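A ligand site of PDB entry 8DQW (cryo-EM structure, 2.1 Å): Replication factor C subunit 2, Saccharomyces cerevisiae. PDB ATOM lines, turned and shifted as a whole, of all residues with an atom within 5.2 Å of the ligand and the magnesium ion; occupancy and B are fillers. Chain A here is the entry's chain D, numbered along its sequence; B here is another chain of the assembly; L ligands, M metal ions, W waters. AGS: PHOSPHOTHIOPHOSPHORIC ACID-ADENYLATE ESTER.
Water W4 lies within hydrogen-bond range of OD2 of Asp 140, OE2 of Glu 141 and NH2 of Arg 184 of chain B.
Water W2 lies within hydrogen-bond range of OE1 of Glu 159 of chain B (2.5 Å), NH2 of Arg 184 of chain B (3.3 Å) and NH2 of Arg 229 (3.3 Å).
Water W1 lies within hydrogen-bond range of OD1 of Asp 140 and O3G of the ligand.
Water W3 lies within hydrogen-bond range of a nitrogen (N3) of the ligand (2.8 Å), the backbone carbonyl oxygen of Tyr 31 (2.8 Å) and the guanidinium group of Arg 200 (3.1 Å).
Water W5 lies within hydrogen-bond range of OD1 of Asn 171, O3G of the ligand and NH2 of Arg 155 of chain B.
The backbone NH (N) of Gly 70 is in hydrogen-bond range of a nitrogen (N7) of the ligand (3.1 Å).
NH1 of Arg 32 is in salt-bridge range of O2A of the ligand (3.3 Å).
The backbone NH of Ser 73 is in hydrogen-bond range of an oxygen (O1A) of the ligand, 3.0 Å away.
A nitrogen (N6) of the ligand lies within hydrogen-bond range of the backbone carbonyl oxygen of Thr 69 (3.2 Å).
The backbone NH (N) of Thr 69 lies within hydrogen-bond range of an oxygen (O1B) of the ligand, at 3.2 Å.
An oxygen (O3B) of the ligand lies within hydrogen-bond range of the backbone NH (N) of Gly 68, 3.0 Å away.
OG of Ser 73 lies within hydrogen-bond range of O1A of the ligand.
The guanidinium group (NH1) of Arg 184 of chain B sits close to a sulfur (S1G) of the ligand (3.2 Å).
The backbone NH (N) of Thr 72 sits close to an oxygen (O2B) of the ligand.
An oxygen (O1B) of the ligand lies within salt-bridge range of the side-chain amino group of Lys 71, at 2.6 Å.
An oxygen (O2A) of the ligand is in salt-bridge range of the guanidinium group of Arg 229 (3.3 Å).
The backbone carbonyl oxygen of Tyr 31 sits at hydrogen-bond distance from an oxygen (O2') of the ligand (3.5 Å).
OG1 of Thr 69 sits at hydrogen-bond distance from O1B of the ligand (3.4 Å).
The backbone carbonyl oxygen of Val 28 is in hydrogen-bond range of an oxygen (O3') of the ligand (2.7 Å).
The backbone NH of Lys 71 lies within hydrogen-bond range of an oxygen (O1B) of the ligand, 3.3 Å away.
ND2 of Asn 171 sits at hydrogen-bond distance from O3G of the ligand, 3.0 Å away.
N1 of the ligand lies within hydrogen-bond range of N of Thr 40, 3.5 Å away.
An oxygen (O2G) of the ligand sits close to the guanidinium group of Arg 155 of chain B, at 3.0 Å.
N6 of the ligand sits at hydrogen-bond distance from O of Thr 40 (3.1 Å).
Of the 32 residues printed, 1 comes within 4 Å of the magnesium ion.
The magnesium ion is bound by water W4, O2B of the ligand, O2G of the ligand, water W1, OG1 of Thr 72 and water W2.
The magnesium ion has six donor atoms within binding distance.
OE2 of Glu 159 of chain B sits close to O2A of the ligand (3.2 Å).
Residues that only touch the ligand: Pro 33 (3.6 Å), Val 39 (3.7 Å), Pro 67 (3.6 Å), Leu 192 (3.6 Å), Leu 228 (3.6 Å), Ile 232 (3.8 Å) and Pro 180 of chain B (3.7 Å).
Hydrophobic or aromatic side chains that line the ligand: Pro 33, Val 39, Pro 67, Leu 192, Leu 228, Ile 232 and Pro 180 of chain B.
22 residues have an atom within 4 Å of the ligand: Val 28, Tyr 31, Arg 32, Pro 33, Val 39, Thr 40, Pro 67, Gly 68, Thr 69, Gly 70, Lys 71, Thr 72, Ser 73, Asn 171, Leu 192, Leu 228, Arg 229, Ile 232, Arg 155 of chain B, Glu 159 of chain B, Pro 180 of chain B and Arg 184 of chain B.
The side-chain amino group (NZ) of Lys 71 is in hydrogen-bond range of the side-chain hydroxyl (OG1) of Thr 69, at 3.3 Å.
NZ of Lys 71 lies within hydrogen-bond range of O of Gly 65, at 3.2 Å.
The side-chain hydroxyl of Ser 73 is in hydrogen-bond range of the guanidinium group of Arg 32, 2.6 Å away.
OE2 of Glu 159 of chain B is in salt-bridge range of NH2 of Arg 32, at 2.8 Å.
The side-chain hydroxyl (OG1) of Thr 69 sits at hydrogen-bond distance from the backbone carbonyl oxygen (O) of Pro 66 (3.0 Å).
The side-chain amino group (NZ) of Lys 71 lies within hydrogen-bond range of the backbone carbonyl oxygen (O) of Pro 66, 3.1 Å away.
The guanidinium group (NE) of Arg 32 lies within salt-bridge range of the side-chain carboxylate (OE1) of Glu 29, 3.3 Å away.
OD2 of Asp 140 sits close to OG1 of Thr 72, 2.9 Å away.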
ATOM      1  N   TRP A  27      -2.795   0.915  -3.256  1.00  0.00           N
ATOM      2  CA  TRP A  27      -1.876   1.530  -2.305  1.00  0.00           C
ATOM      3  C   TRP A  27      -1.209   2.772  -2.878  1.00  0.00           C
ATOM      4  O   TRP A  27      -0.888   3.701  -2.131  1.00  0.00           O
ATOM      5  CB  TRP A  27      -0.823   0.514  -1.872  1.00  0.00           C
ATOM      6  CG  TRP A  27      -1.360  -0.532  -0.930  1.00  0.00           C
ATOM      7  CD1 TRP A  27      -2.669  -0.767  -0.632  1.00  0.00           C
ATOM      8  CD2 TRP A  27      -0.598  -1.479  -0.169  1.00  0.00           C
ATOM      9  NE1 TRP A  27      -2.775  -1.801   0.264  1.00  0.00           N
ATOM     10  CE2 TRP A  27      -1.518  -2.258   0.569  1.00  0.00           C
ATOM     11  CE3 TRP A  27       0.763  -1.750  -0.051  1.00  0.00           C
ATOM     12  CZ2 TRP A  27      -1.116  -3.289   1.413  1.00  0.00           C
ATOM     13  CZ3 TRP A  27       1.169  -2.768   0.791  1.00  0.00           C
ATOM     14  CH2 TRP A  27       0.233  -3.525   1.512  1.00  0.00           C
ATOM     15  N   VAL A  28      -1.009   2.816  -4.205  1.00  0.00           N
ATOM     16  CA  VAL A  28      -0.384   3.985  -4.813  1.00  0.00           C
ATOM     17  C   VAL A  28      -1.265   5.211  -4.647  1.00  0.00           C
ATOM     18  O   VAL A  28      -0.798   6.306  -4.333  1.00  0.00           O
ATOM     19  CB  VAL A  28      -0.043   3.716  -6.289  1.00  0.00           C
ATOM     20  CG1 VAL A  28       1.040   2.639  -6.392  1.00  0.00           C
ATOM     21  CG2 VAL A  28      -1.282   3.310  -7.080  1.00  0.00           C
ATOM     22  N   GLU A  29      -2.577   5.050  -4.867  1.00  0.00           N
ATOM     23  CA  GLU A  29      -3.512   6.154  -4.666  1.00  0.00           C
ATOM     24  C   GLU A  29      -3.777   6.381  -3.182  1.00  0.00           C
ATOM     25  O   GLU A  29      -3.926   7.523  -2.740  1.00  0.00           O
ATOM     26  CB  GLU A  29      -4.815   5.887  -5.413  1.00  0.00           C
ATOM     27  CG  GLU A  29      -4.689   5.923  -6.926  1.00  0.00           C
ATOM     28  CD  GLU A  29      -4.020   7.182  -7.443  1.00  0.00           C
ATOM     29  OE1 GLU A  29      -4.234   8.260  -6.832  1.00  0.00           O
ATOM     30  OE2 GLU A  29      -3.290   7.101  -8.450  1.00  0.00           O
ATOM     31  N   TYR A  31      -1.752   6.017  -0.632  1.00  0.00           N
ATOM     32  CA  TYR A  31      -0.618   6.670   0.011  1.00  0.00           C
ATOM     33  C   TYR A  31      -0.021   7.781  -0.841  1.00  0.00           C
ATOM     34  O   TYR A  31       1.163   8.109  -0.681  1.00  0.00           O
ATOM     35  CB  TYR A  31       0.443   5.630   0.367  1.00  0.00           C
ATOM     36  CG  TYR A  31       0.020   4.734   1.509  1.00  0.00           C
ATOM     37  CD1 TYR A  31       0.047   5.187   2.823  1.00  0.00           C
ATOM     38  CD2 TYR A  31      -0.430   3.444   1.267  1.00  0.00           C
ATOM     39  CE1 TYR A  31      -0.346   4.369   3.874  1.00  0.00           C
ATOM     40  CE2 TYR A  31      -0.819   2.617   2.309  1.00  0.00           C
ATOM     41  CZ  TYR A  31      -0.775   3.084   3.602  1.00  0.00           C
ATOM     42  OH  TYR A  31      -1.174   2.266   4.641  1.00  0.00           O
ATOM     43  N   ARG A  32      -0.798   8.365  -1.745  1.00  0.00           N
ATOM     44  CA  ARG A  32      -0.327   9.543  -2.459  1.00  0.00           C
ATOM     45  C   ARG A  32      -0.109  10.687  -1.468  1.00  0.00           C
ATOM     46  O   ARG A  32      -0.980  10.925  -0.621  1.00  0.00           O
ATOM     47  CB  ARG A  32      -1.326   9.966  -3.538  1.00  0.00           C
ATOM     48  CG  ARG A  32      -0.876  11.152  -4.373  1.00  0.00           C
ATOM     49  CD  ARG A  32      -1.921  11.558  -5.399  1.00  0.00           C
ATOM     50  NE  ARG A  32      -1.985  10.628  -6.526  1.00  0.00           N
ATOM     51  CZ  ARG A  32      -1.068  10.532  -7.470  1.00  0.00           C
ATOM     52  NH1 ARG A  32       0.027  11.293  -7.467  1.00  0.00           N
ATOM     53  NH2 ARG A  32      -1.235   9.664  -8.457  1.00  0.00           N
ATOM     54  N   PRO A  33       1.019  11.394  -1.521  1.00  0.00           N
ATOM     55  CA  PRO A  33       1.270  12.445  -0.526  1.00  0.00           C
ATOM     56  C   PRO A  33       0.135  13.454  -0.478  1.00  0.00           C
ATOM     57  O   PRO A  33      -0.380  13.890  -1.512  1.00  0.00           O
ATOM     58  CB  PRO A  33       2.583  13.083  -1.009  1.00  0.00           C
ATOM     59  CG  PRO A  33       3.246  12.023  -1.803  1.00  0.00           C
ATOM     60  CD  PRO A  33       2.164  11.208  -2.439  1.00  0.00           C
ATOM     61  N   GLU A  38       5.020  15.243   2.905  1.00  0.00           N
ATOM     62  CA  GLU A  38       5.002  13.817   2.611  1.00  0.00           C
ATOM     63  C   GLU A  38       5.833  13.448   1.394  1.00  0.00           C
ATOM     64  O   GLU A  38       6.193  12.270   1.232  1.00  0.00           O
ATOM     65  CB  GLU A  38       3.555  13.340   2.408  1.00  0.00           C
ATOM     66  CG  GLU A  38       2.773  13.179   3.699  1.00  0.00           C
ATOM     67  CD  GLU A  38       1.684  12.125   3.592  1.00  0.00           C
ATOM     68  OE1 GLU A  38       0.595  12.442   3.073  1.00  0.00           O
ATOM     69  OE2 GLU A  38       1.929  10.976   4.019  1.00  0.00           O
ATOM     70  N   VAL A  39       6.153  14.412   0.532  1.00  0.00           N
ATOM     71  CA  VAL A  39       6.997  14.132  -0.627  1.00  0.00           C
ATOM     72  C   VAL A  39       8.408  13.819  -0.154  1.00  0.00           C
ATOM     73  O   VAL A  39       8.980  14.536   0.683  1.00  0.00           O
ATOM     74  CB  VAL A  39       6.990  15.310  -1.608  1.00  0.00           C
ATOM     75  CG1 VAL A  39       7.837  15.003  -2.832  1.00  0.00           C
ATOM     76  CG2 VAL A  39       5.560  15.639  -2.021  1.00  0.00           C
ATOM     77  N   THR A  40       8.983  12.741  -0.678  1.00  0.00           N
ATOM     78  CA  THR A  40      10.290  12.255  -0.252  1.00  0.00           C
ATOM     79  C   THR A  40      11.305  12.360  -1.380  1.00  0.00           C
ATOM     80  O   THR A  40      10.964  12.241  -2.565  1.00  0.00           O
ATOM     81  CB  THR A  40      10.194  10.798   0.225  1.00  0.00           C
ATOM     82  OG1 THR A  40      11.320  10.495   1.069  1.00  0.00           O
ATOM     83  CG2 THR A  40      10.183   9.826  -0.955  1.00  0.00           C
ATOM     84  N   GLN A  42      12.905  14.653  -2.854  1.00  0.00           N
ATOM     85  CA  GLN A  42      12.909  15.763  -3.802  1.00  0.00           C
ATOM     86  C   GLN A  42      12.980  17.098  -3.061  1.00  0.00           C
ATOM     87  O   GLN A  42      12.337  18.082  -3.450  1.00  0.00           O
ATOM     88  CB  GLN A  42      11.669  15.711  -4.696  1.00  0.00           C
ATOM     89  CG  GLN A  42      11.336  14.317  -5.241  1.00  0.00           C
ATOM     90  CD  GLN A  42      12.378  13.807  -6.227  1.00  0.00           C
ATOM     91  OE1 GLN A  42      13.519  14.268  -6.251  1.00  0.00           O
ATOM     92  NE2 GLN A  42      11.980  12.834  -7.040  1.00  0.00           N
ATOM     93  N   GLY A  65      11.068  14.613 -15.154  1.00  0.00           N
ATOM     94  CA  GLY A  65      11.713  13.462 -14.571  1.00  0.00           C
ATOM     95  C   GLY A  65      11.124  12.118 -14.964  1.00  0.00           C
ATOM     96  O   GLY A  65      10.071  12.037 -15.604  1.00  0.00           O
ATOM     97  N   PRO A  66      11.786  11.040 -14.554  1.00  0.00           N
ATOM     98  CA  PRO A  66      11.356   9.692 -14.961  1.00  0.00           C
ATOM     99  C   PRO A  66      10.066   9.288 -14.271  1.00  0.00           C
ATOM    100  O   PRO A  66       9.608   9.970 -13.338  1.00  0.00           O
ATOM    101  CB  PRO A  66      12.531   8.796 -14.545  1.00  0.00           C
ATOM    102  CG  PRO A  66      13.343   9.581 -13.577  1.00  0.00           C
ATOM    103  CD  PRO A  66      12.980  11.029 -13.685  1.00  0.00           C
ATOM    104  N   PRO A  67       9.466   8.184 -14.686  1.00  0.00           N
ATOM    105  CA  PRO A  67       8.135   7.826 -14.174  1.00  0.00           C
ATOM    106  C   PRO A  67       8.121   7.584 -12.670  1.00  0.00           C
ATOM    107  O   PRO A  67       9.081   7.084 -12.092  1.00  0.00           O
ATOM    108  CB  PRO A  67       7.781   6.547 -14.939  1.00  0.00           C
ATOM    109  CG  PRO A  67       8.731   6.477 -16.088  1.00  0.00           C
ATOM    110  CD  PRO A  67       9.962   7.206 -15.667  1.00  0.00           C
ATOM    111  N   GLY A  68       7.009   7.962 -12.045  1.00  0.00           N
ATOM    112  CA  GLY A  68       6.769   7.654 -10.648  1.00  0.00           C
ATOM    113  C   GLY A  68       7.747   8.269  -9.676  1.00  0.00           C
ATOM    114  O   GLY A  68       8.157   7.620  -8.710  1.00  0.00           O
ATOM    115  N   THR A  69       8.134   9.530  -9.898  1.00  0.00           N
ATOM    116  CA  THR A  69       9.043  10.231  -9.007  1.00  0.00           C
ATOM    117  C   THR A  69       8.362  11.280  -8.135  1.00  0.00           C
ATOM    118  O   THR A  69       9.007  11.796  -7.210  1.00  0.00           O
ATOM    119  CB  THR A  69      10.168  10.900  -9.810  1.00  0.00           C
ATOM    120  OG1 THR A  69       9.611  11.682 -10.872  1.00  0.00           O
ATOM    121  CG2 THR A  69      11.115   9.851 -10.387  1.00  0.00           C
ATOM    122  N   GLY A  70       7.105  11.614  -8.396  1.00  0.00           N
ATOM    123  CA  GLY A  70       6.351  12.468  -7.506  1.00  0.00           C
ATOM    124  C   GLY A  70       6.075  13.867  -8.035  1.00  0.00           C
ATOM    125  O   GLY A  70       5.956  14.814  -7.254  1.00  0.00           O
ATOM    126  N   LYS A  71       5.958  14.002  -9.359  1.00  0.00           N
ATOM    127  CA  LYS A  71       5.717  15.323  -9.953  1.00  0.00           C
ATOM    128  C   LYS A  71       4.257  15.733  -9.800  1.00  0.00           C
ATOM    129  O   LYS A  71       3.943  16.795  -9.250  1.00  0.00           O
ATOM    130  CB  LYS A  71       6.129  15.296 -11.435  1.00  0.00           C
ATOM    131  CG  LYS A  71       7.567  14.839 -11.662  1.00  0.00           C
ATOM    132  CD  LYS A  71       7.983  14.947 -13.125  1.00  0.00           C
ATOM    133  CE  LYS A  71       7.360  13.849 -13.973  1.00  0.00           C
ATOM    134  NZ  LYS A  71       7.716  12.474 -13.503  1.00  0.00           N
ATOM    135  N   THR A  72       3.337  14.888 -10.283  1.00  0.00           N
ATOM    136  CA  THR A  72       1.911  15.183 -10.157  1.00  0.00           C
ATOM    137  C   THR A  72       1.516  15.329  -8.687  1.00  0.00           C
ATOM    138  O   THR A  72       0.763  16.248  -8.324  1.00  0.00           O
ATOM    139  CB  THR A  72       1.089  14.077 -10.827  1.00  0.00           C
ATOM    140  OG1 THR A  72       1.317  14.106 -12.243  1.00  0.00           O
ATOM    141  CG2 THR A  72      -0.392  14.259 -10.551  1.00  0.00           C
ATOM    142  N   SER A  73       2.018  14.443  -7.831  1.00  0.00           N
ATOM    143  CA  SER A  73       1.715  14.540  -6.405  1.00  0.00           C
ATOM    144  C   SER A  73       2.209  15.864  -5.836  1.00  0.00           C
ATOM    145  O   SER A  73       1.513  16.512  -5.047  1.00  0.00           O
ATOM    146  CB  SER A  73       2.334  13.363  -5.647  1.00  0.00           C
ATOM    147  OG  SER A  73       2.189  12.151  -6.353  1.00  0.00           O
ATOM    148  N   THR A  74       3.424  16.276  -6.225  1.00  0.00           N
ATOM    149  CA  THR A  74       3.975  17.521  -5.701  1.00  0.00           C
ATOM    150  C   THR A  74       3.121  18.716  -6.111  1.00  0.00           C
ATOM    151  O   THR A  74       2.821  19.581  -5.289  1.00  0.00           O
ATOM    152  CB  THR A  74       5.417  17.693  -6.190  1.00  0.00           C
ATOM    153  OG1 THR A  74       6.244  16.686  -5.596  1.00  0.00           O
ATOM    154  CG2 THR A  74       5.948  19.075  -5.814  1.00  0.00           C
ATOM    155  N   ASP A 140      -0.185  18.930 -17.386  1.00  0.00           N
ATOM    156  CA  ASP A 140       0.459  17.646 -17.147  1.00  0.00           C
ATOM    157  C   ASP A 140       0.690  16.915 -18.469  1.00  0.00           C
ATOM    158  O   ASP A 140      -0.041  17.098 -19.434  1.00  0.00           O
ATOM    159  CB  ASP A 140      -0.403  16.793 -16.207  1.00  0.00           C
ATOM    160  CG  ASP A 140       0.420  15.827 -15.373  1.00  0.00           C
ATOM    161  OD1 ASP A 140       1.646  15.709 -15.609  1.00  0.00           O
ATOM    162  OD2 ASP A 140      -0.157  15.185 -14.465  1.00  0.00           O
ATOM    163  N   GLU A 141       1.726  16.077 -18.488  1.00  0.00           N
ATOM    164  CA  GLU A 141       2.111  15.382 -19.707  1.00  0.00           C
ATOM    165  C   GLU A 141       2.312  16.371 -20.848  1.00  0.00           C
ATOM    166  O   GLU A 141       1.883  16.147 -21.986  1.00  0.00           O
ATOM    167  CB  GLU A 141       1.079  14.309 -20.079  1.00  0.00           C
ATOM    168  CG  GLU A 141       1.107  13.088 -19.183  1.00  0.00           C
ATOM    169  CD  GLU A 141      -0.215  12.818 -18.476  1.00  0.00           C
ATOM    170  OE1 GLU A 141      -1.274  13.198 -19.018  1.00  0.00           O
ATOM    171  OE2 GLU A 141      -0.191  12.224 -17.381  1.00  0.00           O
ATOM    172  N   ASN A 171       8.145  13.882 -18.760  1.00  0.00           N
ATOM    173  CA  ASN A 171       9.190  12.880 -18.596  1.00  0.00           C
ATOM    174  C   ASN A 171      10.360  13.102 -19.539  1.00  0.00           C
ATOM    175  O   ASN A 171      11.498  12.792 -19.166  1.00  0.00           O
ATOM    176  CB  ASN A 171       8.616  11.477 -18.829  1.00  0.00           C
ATOM    177  CG  ASN A 171       7.494  11.140 -17.865  1.00  0.00           C
ATOM    178  OD1 ASN A 171       6.314  11.276 -18.198  1.00  0.00           O
ATOM    179  ND2 ASN A 171       7.850  10.694 -16.667  1.00  0.00           N
ATOM    180  N   LEU A 192      13.966   7.487  -7.632  1.00  0.00           N
ATOM    181  CA  LEU A 192      13.749   7.029  -6.261  1.00  0.00           C
ATOM    182  C   LEU A 192      14.289   5.611  -6.131  1.00  0.00           C
ATOM    183  O   LEU A 192      13.735   4.666  -6.694  1.00  0.00           O
ATOM    184  CB  LEU A 192      12.260   7.088  -5.912  1.00  0.00           C
ATOM    185  CG  LEU A 192      11.595   8.455  -6.087  1.00  0.00           C
ATOM    186  CD1 LEU A 192      10.144   8.409  -5.636  1.00  0.00           C
ATOM    187  CD2 LEU A 192      12.360   9.530  -5.330  1.00  0.00           C
ATOM    188  N   ARG A 200       9.883   5.942   3.063  1.00  0.00           N
ATOM    189  CA  ARG A 200       8.466   5.965   2.709  1.00  0.00           C
ATOM    190  C   ARG A 200       7.910   4.554   2.533  1.00  0.00           C
ATOM    191  O   ARG A 200       6.807   4.253   2.993  1.00  0.00           O
ATOM    192  CB  ARG A 200       8.261   6.784   1.431  1.00  0.00           C
ATOM    193  CG  ARG A 200       6.803   6.960   1.031  1.00  0.00           C
ATOM    194  CD  ARG A 200       6.054   7.847   2.015  1.00  0.00           C
ATOM    195  NE  ARG A 200       4.739   8.229   1.503  1.00  0.00           N
ATOM    196  CZ  ARG A 200       3.705   8.582   2.257  1.00  0.00           C
ATOM    197  NH1 ARG A 200       3.795   8.629   3.583  1.00  0.00           N
ATOM    198  NH2 ARG A 200       2.553   8.884   1.678  1.00  0.00           N
ATOM    199  N   LEU A 228       8.958   4.607  -7.643  1.00  0.00           N
ATOM    200  CA  LEU A 228       8.365   4.232  -6.367  1.00  0.00           C
ATOM    201  C   LEU A 228       6.953   3.682  -6.535  1.00  0.00           C
ATOM    202  O   LEU A 228       6.501   2.874  -5.714  1.00  0.00           O
ATOM    203  CB  LEU A 228       8.373   5.417  -5.409  1.00  0.00           C
ATOM    204  CG  LEU A 228       7.822   5.200  -3.997  1.00  0.00           C
ATOM    205  CD1 LEU A 228       8.492   4.006  -3.309  1.00  0.00           C
ATOM    206  CD2 LEU A 228       7.994   6.447  -3.161  1.00  0.00           C
ATOM    207  N   ARG A 229       6.243   4.117  -7.575  1.00  0.00           N
ATOM    208  CA  ARG A 229       4.911   3.590  -7.844  1.00  0.00           C
ATOM    209  C   ARG A 229       4.959   2.085  -8.104  1.00  0.00           C
ATOM    210  O   ARG A 229       4.170   1.310  -7.554  1.00  0.00           O
ATOM    211  CB  ARG A 229       4.295   4.324  -9.023  1.00  0.00           C
ATOM    212  CG  ARG A 229       2.791   4.154  -9.176  1.00  0.00           C
ATOM    213  CD  ARG A 229       2.352   4.301 -10.630  1.00  0.00           C
ATOM    214  NE  ARG A 229       1.928   5.662 -10.942  1.00  0.00           N
ATOM    215  CZ  ARG A 229       2.629   6.532 -11.654  1.00  0.00           C
ATOM    216  NH1 ARG A 229       3.798   6.228 -12.179  1.00  0.00           N
ATOM    217  NH2 ARG A 229       2.133   7.759 -11.854  1.00  0.00           N
ATOM    218  N   ILE A 232       5.645   0.267  -4.813  1.00  0.00           N
ATOM    219  CA  ILE A 232       4.466   0.171  -3.951  1.00  0.00           C
ATOM    220  C   ILE A 232       3.507  -0.884  -4.493  1.00  0.00           C
ATOM    221  O   ILE A 232       2.925  -1.663  -3.728  1.00  0.00           O
ATOM    222  CB  ILE A 232       3.788   1.542  -3.820  1.00  0.00           C
ATOM    223  CG1 ILE A 232       4.639   2.487  -2.972  1.00  0.00           C
ATOM    224  CG2 ILE A 232       2.404   1.399  -3.203  1.00  0.00           C
ATOM    225  CD1 ILE A 232       4.330   3.949  -3.180  1.00  0.00           C
ATOM    226  N   ARG B 155      -3.212   7.712 -18.923  1.00  0.00           N
ATOM    227  CA  ARG B 155      -2.493   7.825 -17.660  1.00  0.00           C
ATOM    228  C   ARG B 155      -3.348   8.488 -16.576  1.00  0.00           C
ATOM    229  O   ARG B 155      -3.640   7.892 -15.530  1.00  0.00           O
ATOM    230  CB  ARG B 155      -1.196   8.600 -17.871  1.00  0.00           C
ATOM    231  CG  ARG B 155      -0.193   7.886 -18.776  1.00  0.00           C
ATOM    232  CD  ARG B 155       0.845   8.848 -19.368  1.00  0.00           C
ATOM    233  NE  ARG B 155       1.453   9.723 -18.366  1.00  0.00           N
ATOM    234  CZ  ARG B 155       2.643  10.274 -18.478  1.00  0.00           C
ATOM    235  NH1 ARG B 155       3.403  10.088 -19.544  1.00  0.00           N
ATOM    236  NH2 ARG B 155       3.104  11.056 -17.496  1.00  0.00           N
ATOM    237  N   GLU B 159      -5.292   7.199 -13.130  1.00  0.00           N
ATOM    238  CA  GLU B 159      -4.918   7.669 -11.804  1.00  0.00           C
ATOM    239  C   GLU B 159      -6.074   8.360 -11.088  1.00  0.00           C
ATOM    240  O   GLU B 159      -6.469   7.973  -9.979  1.00  0.00           O
ATOM    241  CB  GLU B 159      -3.717   8.611 -11.897  1.00  0.00           C
ATOM    242  CG  GLU B 159      -2.377   7.889 -11.927  1.00  0.00           C
ATOM    243  CD  GLU B 159      -1.213   8.837 -11.799  1.00  0.00           C
ATOM    244  OE1 GLU B 159      -1.141   9.803 -12.594  1.00  0.00           O
ATOM    245  OE2 GLU B 159      -0.359   8.623 -10.915  1.00  0.00           O
ATOM    246  N   PRO B 180       5.299   4.793 -18.586  1.00  0.00           N
ATOM    247  CA  PRO B 180       4.311   5.215 -17.584  1.00  0.00           C
ATOM    248  C   PRO B 180       3.160   4.220 -17.418  1.00  0.00           C
ATOM    249  O   PRO B 180       2.734   3.960 -16.285  1.00  0.00           O
ATOM    250  CB  PRO B 180       3.807   6.559 -18.128  1.00  0.00           C
ATOM    251  CG  PRO B 180       4.898   7.049 -19.019  1.00  0.00           C
ATOM    252  CD  PRO B 180       5.533   5.822 -19.609  1.00  0.00           C
ATOM    253  N   ARG B 184       2.004   2.136 -14.051  1.00  0.00           N
ATOM    254  CA  ARG B 184       0.680   2.246 -13.466  1.00  0.00           C
ATOM    255  C   ARG B 184      -0.039   0.904 -13.341  1.00  0.00           C
ATOM    256  O   ARG B 184      -1.230   0.884 -12.992  1.00  0.00           O
ATOM    257  CB  ARG B 184      -0.183   3.198 -14.299  1.00  0.00           C
ATOM    258  CG  ARG B 184       0.150   4.666 -14.083  1.00  0.00           C
ATOM    259  CD  ARG B 184      -0.519   5.531 -15.134  1.00  0.00           C
ATOM    260  NE  ARG B 184      -0.474   6.947 -14.790  1.00  0.00           N
ATOM    261  CZ  ARG B 184       0.619   7.687 -14.818  1.00  0.00           C
ATOM    262  NH1 ARG B 184       1.793   7.189 -15.172  1.00  0.00           N
ATOM    263  NH2 ARG B 184       0.541   8.966 -14.470  1.00  0.00           N
HETATM  264  PG  AGS L   1       4.505  10.072 -14.194  1.00  0.00           P
HETATM  265  S1G AGS L   1       4.755   8.399 -15.109  1.00  0.00           S
HETATM  266  O2G AGS L   1       2.975  10.641 -14.492  1.00  0.00           O
HETATM  267  O3G AGS L   1       5.645  11.191 -14.711  1.00  0.00           O
HETATM  268  PB  AGS L   1       4.881  10.985 -11.448  1.00  0.00           P
HETATM  269  O1B AGS L   1       6.284  11.572 -11.542  1.00  0.00           O
HETATM  270  O2B AGS L   1       3.847  12.077 -11.659  1.00  0.00           O
HETATM  271  O3B AGS L   1       4.666   9.804 -12.579  1.00  0.00           O
HETATM  272  PA  AGS L   1       3.373  10.515  -9.080  1.00  0.00           P
HETATM  273  O1A AGS L   1       3.401  11.883  -8.472  1.00  0.00           O
HETATM  274  O2A AGS L   1       2.118  10.362  -9.906  1.00  0.00           O
HETATM  275  O3A AGS L   1       4.679  10.299  -9.993  1.00  0.00           O
HETATM  276  O5' AGS L   1       3.393   9.349  -7.876  1.00  0.00           O
HETATM  277  C5' AGS L   1       2.680   8.169  -8.075  1.00  0.00           C
HETATM  278  C4' AGS L   1       2.635   7.396  -6.799  1.00  0.00           C
HETATM  279  O4' AGS L   1       3.806   6.883  -6.529  1.00  0.00           O
HETATM  280  C3' AGS L   1       2.226   8.431  -5.552  1.00  0.00           C
HETATM  281  O3' AGS L   1       0.764   8.350  -5.290  1.00  0.00           O
HETATM  282  C2' AGS L   1       2.869   8.035  -4.566  1.00  0.00           C
HETATM  283  O2' AGS L   1       2.110   6.971  -3.853  1.00  0.00           O
HETATM  284  C1' AGS L   1       4.217   7.418  -5.173  1.00  0.00           C
HETATM  285  N9  AGS L   1       5.194   8.314  -5.342  1.00  0.00           N
HETATM  286  C8  AGS L   1       5.868   8.721  -6.413  1.00  0.00           C
HETATM  287  N7  AGS L   1       6.765   9.626  -6.021  1.00  0.00           N
HETATM  288  C5  AGS L   1       6.645   9.778  -4.701  1.00  0.00           C
HETATM  289  C6  AGS L   1       7.314  10.584  -3.805  1.00  0.00           C
HETATM  290  N6  AGS L   1       8.391  11.528  -4.113  1.00  0.00           N
HETATM  291  N1  AGS L   1       6.997  10.547  -2.517  1.00  0.00           N
HETATM  292  C2  AGS L   1       6.021   9.722  -2.098  1.00  0.00           C
HETATM  293  N3  AGS L   1       5.369   8.932  -2.972  1.00  0.00           N
HETATM  294  C4  AGS L   1       5.687   8.966  -4.277  1.00  0.00           C
HETATM  295 MG    MG M   1       2.347  12.291 -13.163  1.00  0.00          MG
HETATM  296  O   HOH W   1       3.319  13.482 -14.812  1.00  0.00           O
HETATM  297  O   HOH W   2       1.047  10.871 -11.877  1.00  0.00           O
HETATM  298  O   HOH W   3       3.761   7.399  -1.333  1.00  0.00           O
HETATM  299  O   HOH W   4       0.842  12.378 -14.464  1.00  0.00           O
HETATM  300  O   HOH W   5       5.143  13.517 -16.921  1.00  0.00           O
